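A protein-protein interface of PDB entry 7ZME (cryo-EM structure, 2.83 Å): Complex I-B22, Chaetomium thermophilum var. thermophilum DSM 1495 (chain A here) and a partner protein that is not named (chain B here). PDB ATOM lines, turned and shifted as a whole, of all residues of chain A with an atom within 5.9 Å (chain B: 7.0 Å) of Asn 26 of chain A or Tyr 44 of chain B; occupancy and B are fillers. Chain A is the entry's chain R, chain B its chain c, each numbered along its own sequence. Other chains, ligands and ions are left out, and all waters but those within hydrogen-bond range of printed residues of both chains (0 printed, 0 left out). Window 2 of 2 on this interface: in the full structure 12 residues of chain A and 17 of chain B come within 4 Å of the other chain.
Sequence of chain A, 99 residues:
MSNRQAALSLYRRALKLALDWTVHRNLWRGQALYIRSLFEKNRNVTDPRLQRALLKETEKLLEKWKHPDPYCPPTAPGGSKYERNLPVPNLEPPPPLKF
Of the 16 printed residues of chain B, 7 touch a printed residue of chain A. Hydrophobic or aromatic side chains of chain B within 4 Å of the printed part of chain A: Pro 31 and Tyr 44. Printed residues of chain A that touch a printed residue of chain B: Arg 25, Asn 26, Leu 27 and Gly 30.
The side-chain carboxylate of Glu 40 of chain B lies within salt-bridge range of the guanidinium group of Arg 43 of chain B (3.1 Å).
Arg 25 of chain A touches Tyr 44 of chain B. OD1 of Asn 26 of chain A touches CG2 of Thr 30 of chain B (3.8 Å). Thr 28 of chain B touches Leu 27 of chain A. Leu 27 of chain A touches Lys 29 of chain B (CD1 to N, 3.5 Å). Gly 30 of chain A touches Lys 29 of chain B (N to O, 3.7 Å). Gly 30 of chain A touches Pro 31 of chain B.
The guanidinium group (NH2) of Arg 25 of chain A is in salt-bridge range of the side-chain carboxylate (OE2) of Glu 40 of chain B. OH of Tyr 44 of chain B lies close to OD1 of Asn 26 of chain A (3.2 Å). The guanidinium group (NE) of Arg 25 of chain A sits close to the guanidinium group (NH2) of Arg 43 of chain B (3.4 Å). O of Asn 26 of chain A sits close to O of Lys 29 of chain B (3.3 Å).
Of chain B, only Lys 29 (3.3 Å), Thr 30 (3.8 Å) and Tyr 44 (2.9 Å) come within 4 Å of Asn 26 of chain A. Tyr 44 of chain B touches just these residues of chain A: Arg 25 (3.7 Å) and Asn 26 (2.9 Å). Of the printed residues of chain A, Lys 29 of chain B touches Asn 26, Leu 27 and Gly 30. Of the printed residues of chain A, Thr 30 of chain B touches Asn 26 (3.8 Å). Trp 28 of chain A touches none of the printed residues of chain B. Phe 48 of chain B touches none of the printed residues of chain A. The nearest residue of chain B that does not touch Asn 26 of chain A is Pro 31 of chain B (4.4 Å). The nearest residue of chain A that does not touch Tyr 44 of chain B is His 24 of chain A (5.6 Å). The nearest printed residue of chain A that does not touch Arg 43 of chain B is Asn 26 of chain A (6.8 Å).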
ATOM      1  N   HIS A  24       5.302  21.058 -19.493  1.00  0.00           N
ATOM      2  CA  HIS A  24       5.513  21.643 -18.176  1.00  0.00           C
ATOM      3  C   HIS A  24       5.702  23.149 -18.281  1.00  0.00           C
ATOM      4  O   HIS A  24       6.625  23.624 -18.950  1.00  0.00           O
ATOM      5  CB  HIS A  24       6.712  20.977 -17.515  1.00  0.00           C
ATOM      6  CG  HIS A  24       6.665  19.485 -17.580  1.00  0.00           C
ATOM      7  ND1 HIS A  24       7.794  18.716 -17.756  1.00  0.00           N
ATOM      8  CD2 HIS A  24       5.634  18.617 -17.467  1.00  0.00           C
ATOM      9  CE1 HIS A  24       7.459  17.439 -17.764  1.00  0.00           C
ATOM     10  NE2 HIS A  24       6.154  17.351 -17.591  1.00  0.00           N
ATOM     11  N   ARG A  25       4.807  23.919 -17.655  1.00  0.00           N
ATOM     12  CA  ARG A  25       4.841  25.397 -17.843  1.00  0.00           C
ATOM     13  C   ARG A  25       6.106  25.992 -17.232  1.00  0.00           C
ATOM     14  O   ARG A  25       6.503  27.076 -17.687  1.00  0.00           O
ATOM     15  CB  ARG A  25       3.502  26.036 -17.473  1.00  0.00           C
ATOM     16  CG  ARG A  25       2.346  25.528 -18.320  1.00  0.00           C
ATOM     17  CD  ARG A  25       1.120  26.407 -18.213  1.00  0.00           C
ATOM     18  NE  ARG A  25       1.461  27.818 -18.274  1.00  0.00           N
ATOM     19  CZ  ARG A  25       1.118  28.626 -19.267  1.00  0.00           C
ATOM     20  NH1 ARG A  25       0.426  28.158 -20.289  1.00  0.00           N
ATOM     21  NH2 ARG A  25       1.469  29.898 -19.237  1.00  0.00           N
ATOM     22  N   ASN A  26       6.721  25.315 -16.254  1.00  0.00           N
ATOM     23  CA  ASN A  26       8.010  25.799 -15.770  1.00  0.00           C
ATOM     24  C   ASN A  26       9.025  25.882 -16.899  1.00  0.00           C
ATOM     25  O   ASN A  26       9.772  26.860 -17.006  1.00  0.00           O
ATOM     26  CB  ASN A  26       8.564  24.872 -14.691  1.00  0.00           C
ATOM     27  CG  ASN A  26       7.925  25.084 -13.344  1.00  0.00           C
ATOM     28  OD1 ASN A  26       8.017  26.160 -12.754  1.00  0.00           O
ATOM     29  ND2 ASN A  26       7.317  24.028 -12.818  1.00  0.00           N
ATOM     30  N   LEU A  27       9.064  24.856 -17.746  1.00  0.00           N
ATOM     31  CA  LEU A  27      10.194  24.646 -18.640  1.00  0.00           C
ATOM     32  C   LEU A  27      10.030  25.415 -19.940  1.00  0.00           C
ATOM     33  O   LEU A  27      11.021  25.877 -20.514  1.00  0.00           O
ATOM     34  CB  LEU A  27      10.347  23.152 -18.924  1.00  0.00           C
ATOM     35  CG  LEU A  27      11.091  22.278 -17.907  1.00  0.00           C
ATOM     36  CD1 LEU A  27      12.540  22.679 -17.770  1.00  0.00           C
ATOM     37  CD2 LEU A  27      10.406  22.269 -16.546  1.00  0.00           C
ATOM     38  N   TRP A  28       8.793  25.550 -20.419  1.00  0.00           N
ATOM     39  CA  TRP A  28       8.532  26.360 -21.601  1.00  0.00           C
ATOM     40  C   TRP A  28       8.830  27.828 -21.342  1.00  0.00           C
ATOM     41  O   TRP A  28       9.195  28.559 -22.269  1.00  0.00           O
ATOM     42  CB  TRP A  28       7.080  26.173 -22.039  1.00  0.00           C
ATOM     43  CG  TRP A  28       6.568  27.216 -22.971  1.00  0.00           C
ATOM     44  CD1 TRP A  28       6.881  27.360 -24.282  1.00  0.00           C
ATOM     45  CD2 TRP A  28       5.637  28.257 -22.663  1.00  0.00           C
ATOM     46  NE1 TRP A  28       6.207  28.429 -24.816  1.00  0.00           N
ATOM     47  CE2 TRP A  28       5.436  28.998 -23.840  1.00  0.00           C
ATOM     48  CE3 TRP A  28       4.957  28.637 -21.504  1.00  0.00           C
ATOM     49  CZ2 TRP A  28       4.587  30.094 -23.895  1.00  0.00           C
ATOM     50  CZ3 TRP A  28       4.114  29.724 -21.560  1.00  0.00           C
ATOM     51  CH2 TRP A  28       3.934  30.440 -22.747  1.00  0.00           C
ATOM     52  N   ARG A  29       8.688  28.272 -20.093  1.00  0.00           N
ATOM     53  CA  ARG A  29       8.991  29.659 -19.762  1.00  0.00           C
ATOM     54  C   ARG A  29      10.451  29.978 -20.040  1.00  0.00           C
ATOM     55  O   ARG A  29      10.771  31.046 -20.575  1.00  0.00           O
ATOM     56  CB  ARG A  29       8.642  29.934 -18.302  1.00  0.00           C
ATOM     57  CG  ARG A  29       8.610  31.405 -17.952  1.00  0.00           C
ATOM     58  CD  ARG A  29       7.330  32.055 -18.444  1.00  0.00           C
ATOM     59  NE  ARG A  29       7.576  32.961 -19.561  1.00  0.00           N
ATOM     60  CZ  ARG A  29       6.636  33.694 -20.147  1.00  0.00           C
ATOM     61  NH1 ARG A  29       5.383  33.628 -19.722  1.00  0.00           N
ATOM     62  NH2 ARG A  29       6.948  34.492 -21.159  1.00  0.00           N
ATOM     63  N   GLY A  30      11.354  29.064 -19.687  1.00  0.00           N
ATOM     64  CA  GLY A  30      12.742  29.232 -20.079  1.00  0.00           C
ATOM     65  C   GLY A  30      12.917  29.201 -21.585  1.00  0.00           C
ATOM     66  O   GLY A  30      13.690  29.980 -22.146  1.00  0.00           O
ATOM     67  N   THR B  28      16.407  25.205 -21.082  1.00  0.00           N
ATOM     68  CA  THR B  28      15.203  24.485 -20.684  1.00  0.00           C
ATOM     69  C   THR B  28      15.271  24.294 -19.171  1.00  0.00           C
ATOM     70  O   THR B  28      15.759  23.276 -18.677  1.00  0.00           O
ATOM     71  CB  THR B  28      15.098  23.153 -21.426  1.00  0.00           C
ATOM     72  OG1 THR B  28      15.047  23.396 -22.839  1.00  0.00           O
ATOM     73  CG2 THR B  28      13.852  22.395 -21.009  1.00  0.00           C
ATOM     74  N   LYS B  29      14.787  25.291 -18.438  1.00  0.00           N
ATOM     75  CA  LYS B  29      14.795  25.276 -16.980  1.00  0.00           C
ATOM     76  C   LYS B  29      13.813  26.335 -16.493  1.00  0.00           C
ATOM     77  O   LYS B  29      13.031  26.887 -17.274  1.00  0.00           O
ATOM     78  CB  LYS B  29      16.209  25.511 -16.437  1.00  0.00           C
ATOM     79  N   THR B  30      13.841  26.607 -15.192  1.00  0.00           N
ATOM     80  CA  THR B  30      13.114  27.739 -14.639  1.00  0.00           C
ATOM     81  C   THR B  30      14.022  28.959 -14.654  1.00  0.00           C
ATOM     82  O   THR B  30      15.062  28.949 -13.983  1.00  0.00           O
ATOM     83  CB  THR B  30      12.655  27.450 -13.221  1.00  0.00           C
ATOM     84  OG1 THR B  30      13.795  27.218 -12.385  1.00  0.00           O
ATOM     85  CG2 THR B  30      11.755  26.223 -13.194  1.00  0.00           C
ATOM     86  N   PRO B  31      13.686  30.013 -15.391  1.00  0.00           N
ATOM     87  CA  PRO B  31      14.616  31.142 -15.522  1.00  0.00           C
ATOM     88  C   PRO B  31      14.765  31.896 -14.211  1.00  0.00           C
ATOM     89  O   PRO B  31      13.830  31.984 -13.411  1.00  0.00           O
ATOM     90  CB  PRO B  31      13.976  32.019 -16.605  1.00  0.00           C
ATOM     91  CG  PRO B  31      12.572  31.514 -16.788  1.00  0.00           C
ATOM     92  CD  PRO B  31      12.349  30.314 -15.925  1.00  0.00           C
ATOM     93  N   GLU B  40       2.551  33.892 -13.214  1.00  0.00           N
ATOM     94  CA  GLU B  40       2.753  32.451 -13.289  1.00  0.00           C
ATOM     95  C   GLU B  40       3.049  31.810 -11.941  1.00  0.00           C
ATOM     96  O   GLU B  40       2.967  30.584 -11.826  1.00  0.00           O
ATOM     97  CB  GLU B  40       3.890  32.126 -14.265  1.00  0.00           C
ATOM     98  CG  GLU B  40       3.592  32.472 -15.713  1.00  0.00           C
ATOM     99  CD  GLU B  40       2.485  31.619 -16.299  1.00  0.00           C
ATOM    100  OE1 GLU B  40       2.353  30.447 -15.888  1.00  0.00           O
ATOM    101  OE2 GLU B  40       1.749  32.120 -17.175  1.00  0.00           O
ATOM    102  N   ALA B  41       3.395  32.600 -10.922  1.00  0.00           N
ATOM    103  CA  ALA B  41       3.796  32.029  -9.642  1.00  0.00           C
ATOM    104  C   ALA B  41       2.661  31.304  -8.933  1.00  0.00           C
ATOM    105  O   ALA B  41       2.931  30.456  -8.078  1.00  0.00           O
ATOM    106  CB  ALA B  41       4.355  33.119  -8.726  1.00  0.00           C
ATOM    107  N   TRP B  42       1.405  31.609  -9.268  1.00  0.00           N
ATOM    108  CA  TRP B  42       0.281  30.998  -8.569  1.00  0.00           C
ATOM    109  C   TRP B  42       0.262  29.487  -8.707  1.00  0.00           C
ATOM    110  O   TRP B  42      -0.323  28.805  -7.860  1.00  0.00           O
ATOM    111  CB  TRP B  42      -1.041  31.566  -9.079  1.00  0.00           C
ATOM    112  CG  TRP B  42      -1.455  31.059 -10.429  1.00  0.00           C
ATOM    113  CD1 TRP B  42      -1.242  31.665 -11.630  1.00  0.00           C
ATOM    114  CD2 TRP B  42      -2.172  29.851 -10.715  1.00  0.00           C
ATOM    115  NE1 TRP B  42      -1.776  30.913 -12.645  1.00  0.00           N
ATOM    116  CE2 TRP B  42      -2.352  29.794 -12.109  1.00  0.00           C
ATOM    117  CE3 TRP B  42      -2.674  28.812  -9.930  1.00  0.00           C
ATOM    118  CZ2 TRP B  42      -3.008  28.742 -12.731  1.00  0.00           C
ATOM    119  CZ3 TRP B  42      -3.322  27.770 -10.549  1.00  0.00           C
ATOM    120  CH2 TRP B  42      -3.483  27.741 -11.936  1.00  0.00           C
ATOM    121  N   ARG B  43       0.880  28.951  -9.755  1.00  0.00           N
ATOM    122  CA  ARG B  43       0.835  27.515  -9.976  1.00  0.00           C
ATOM    123  C   ARG B  43       1.709  26.767  -8.985  1.00  0.00           C
ATOM    124  O   ARG B  43       1.431  25.610  -8.668  1.00  0.00           O
ATOM    125  CB  ARG B  43       1.264  27.205 -11.405  1.00  0.00           C
ATOM    126  CG  ARG B  43       0.366  27.849 -12.431  1.00  0.00           C
ATOM    127  CD  ARG B  43       0.754  27.480 -13.832  1.00  0.00           C
ATOM    128  NE  ARG B  43      -0.418  27.140 -14.630  1.00  0.00           N
ATOM    129  CZ  ARG B  43      -0.943  27.930 -15.556  1.00  0.00           C
ATOM    130  NH1 ARG B  43      -2.009  27.540 -16.232  1.00  0.00           N
ATOM    131  NH2 ARG B  43      -0.407  29.116 -15.798  1.00  0.00           N
ATOM    132  N   TYR B  44       2.794  27.378  -8.536  1.00  0.00           N
ATOM    133  CA  TYR B  44       3.716  26.740  -7.599  1.00  0.00           C
ATOM    134  C   TYR B  44       3.537  27.305  -6.190  1.00  0.00           C
ATOM    135  O   TYR B  44       4.427  27.937  -5.621  1.00  0.00           O
ATOM    136  CB  TYR B  44       5.138  26.890  -8.118  1.00  0.00           C
ATOM    137  CG  TYR B  44       5.122  26.748  -9.619  1.00  0.00           C
ATOM    138  CD1 TYR B  44       5.062  25.499 -10.210  1.00  0.00           C
ATOM    139  CD2 TYR B  44       5.125  27.866 -10.445  1.00  0.00           C
ATOM    140  CE1 TYR B  44       5.008  25.363 -11.573  1.00  0.00           C
ATOM    141  CE2 TYR B  44       5.081  27.736 -11.817  1.00  0.00           C
ATOM    142  CZ  TYR B  44       5.027  26.480 -12.376  1.00  0.00           C
ATOM    143  OH  TYR B  44       4.987  26.335 -13.743  1.00  0.00           O
ATOM    144  N   THR B  45       2.353  27.064  -5.625  1.00  0.00           N
ATOM    145  CA  THR B  45       1.980  27.656  -4.345  1.00  0.00           C
ATOM    146  C   THR B  45       1.522  26.608  -3.341  1.00  0.00           C
ATOM    147  O   THR B  45       1.701  25.408  -3.560  1.00  0.00           O
ATOM    148  CB  THR B  45       0.882  28.703  -4.536  1.00  0.00           C
ATOM    149  OG1 THR B  45      -0.235  28.110  -5.212  1.00  0.00           O
ATOM    150  CG2 THR B  45       1.402  29.891  -5.329  1.00  0.00           C
ATOM    151  N   GLY B  46       0.940  27.060  -2.226  1.00  0.00           N
ATOM    152  CA  GLY B  46       0.533  26.134  -1.182  1.00  0.00           C
ATOM    153  C   GLY B  46      -0.440  25.078  -1.669  1.00  0.00           C
ATOM    154  O   GLY B  46      -0.314  23.900  -1.327  1.00  0.00           O
ATOM    155  N   ARG B  47      -1.427  25.483  -2.472  1.00  0.00           N
ATOM    156  CA  ARG B  47      -2.370  24.519  -3.024  1.00  0.00           C
ATOM    157  C   ARG B  47      -1.673  23.532  -3.946  1.00  0.00           C
ATOM    158  O   ARG B  47      -2.020  22.345  -3.977  1.00  0.00           O
ATOM    159  CB  ARG B  47      -3.488  25.246  -3.769  1.00  0.00           C
ATOM    160  CG  ARG B  47      -4.515  24.329  -4.411  1.00  0.00           C
ATOM    161  CD  ARG B  47      -5.308  23.551  -3.381  1.00  0.00           C
ATOM    162  NE  ARG B  47      -6.137  24.422  -2.553  1.00  0.00           N
ATOM    163  CZ  ARG B  47      -6.744  24.031  -1.438  1.00  0.00           C
ATOM    164  NH1 ARG B  47      -7.480  24.889  -0.746  1.00  0.00           N
ATOM    165  NH2 ARG B  47      -6.615  22.781  -1.015  1.00  0.00           N
ATOM    166  N   PHE B  48      -0.682  23.997  -4.699  1.00  0.00           N
ATOM    167  CA  PHE B  48       0.008  23.179  -5.683  1.00  0.00           C
ATOM    168  C   PHE B  48       1.495  23.077  -5.378  1.00  0.00           C
ATOM    169  O   PHE B  48       2.339  23.167  -6.270  1.00  0.00           O
ATOM    170  CB  PHE B  48      -0.211  23.729  -7.084  1.00  0.00           C
ATOM    171  CG  PHE B  48      -1.641  24.043  -7.393  1.00  0.00           C
ATOM    172  CD1 PHE B  48      -2.566  23.028  -7.567  1.00  0.00           C
ATOM    173  CD2 PHE B  48      -2.063  25.353  -7.508  1.00  0.00           C
ATOM    174  CE1 PHE B  48      -3.880  23.317  -7.852  1.00  0.00           C
ATOM    175  CE2 PHE B  48      -3.373  25.643  -7.791  1.00  0.00           C
ATOM    176  CZ  PHE B  48      -4.283  24.625  -7.964  1.00  0.00           C
ATOM    177  N   SER B  49       1.834  22.902  -4.107  1.00  0.00           N
ATOM    178  CA  SER B  49       3.213  22.648  -3.725  1.00  0.00           C
ATOM    179  C   SER B  49       3.577  21.194  -4.002  1.00  0.00           C
ATOM    180  O   SER B  49       2.714  20.328  -4.153  1.00  0.00           O
ATOM    181  CB  SER B  49       3.434  22.975  -2.249  1.00  0.00           C
ATOM    182  OG  SER B  49       4.768  22.698  -1.862  1.00  0.00           O
ATOM    183  N   ARG B  50       4.885  20.934  -4.069  1.00  0.00           N
ATOM    184  CA  ARG B  50       5.359  19.569  -4.274  1.00  0.00           C
ATOM    185  C   ARG B  50       4.889  18.642  -3.163  1.00  0.00           C
ATOM    186  O   ARG B  50       4.739  17.435  -3.383  1.00  0.00           O
ATOM    187  CB  ARG B  50       6.886  19.557  -4.364  1.00  0.00           C
ATOM    188  CG  ARG B  50       7.487  18.207  -4.717  1.00  0.00           C
ATOM    189  CD  ARG B  50       9.001  18.287  -4.799  1.00  0.00           C
ATOM    190  NE  ARG B  50       9.444  19.154  -5.885  1.00  0.00           N
ATOM    191  CZ  ARG B  50       9.578  18.757  -7.145  1.00  0.00           C
ATOM    192  NH1 ARG B  50       9.988  19.610  -8.073  1.00  0.00           N
ATOM    193  NH2 ARG B  50       9.302  17.505  -7.474  1.00  0.00           N
ATOM    194  N   ARG B  53       0.591  18.594  -3.091  1.00  0.00           N
ATOM    195  CA  ARG B  53       0.026  17.907  -4.245  1.00  0.00           C
ATOM    196  C   ARG B  53       0.083  16.398  -4.065  1.00  0.00           C
ATOM    197  O   ARG B  53      -0.808  15.677  -4.527  1.00  0.00           O
ATOM    198  CB  ARG B  53       0.757  18.328  -5.516  1.00  0.00           C
ATOM    199  CG  ARG B  53       0.057  19.426  -6.284  1.00  0.00           C
ATOM    200  CD  ARG B  53       0.808  19.764  -7.550  1.00  0.00           C
ATOM    201  NE  ARG B  53       2.140  20.275  -7.252  1.00  0.00           N
ATOM    202  CZ  ARG B  53       3.218  20.018  -7.980  1.00  0.00           C
ATOM    203  NH1 ARG B  53       4.391  20.525  -7.631  1.00  0.00           N
ATOM    204  NH2 ARG B  53       3.122  19.256  -9.059  1.00  0.00           N
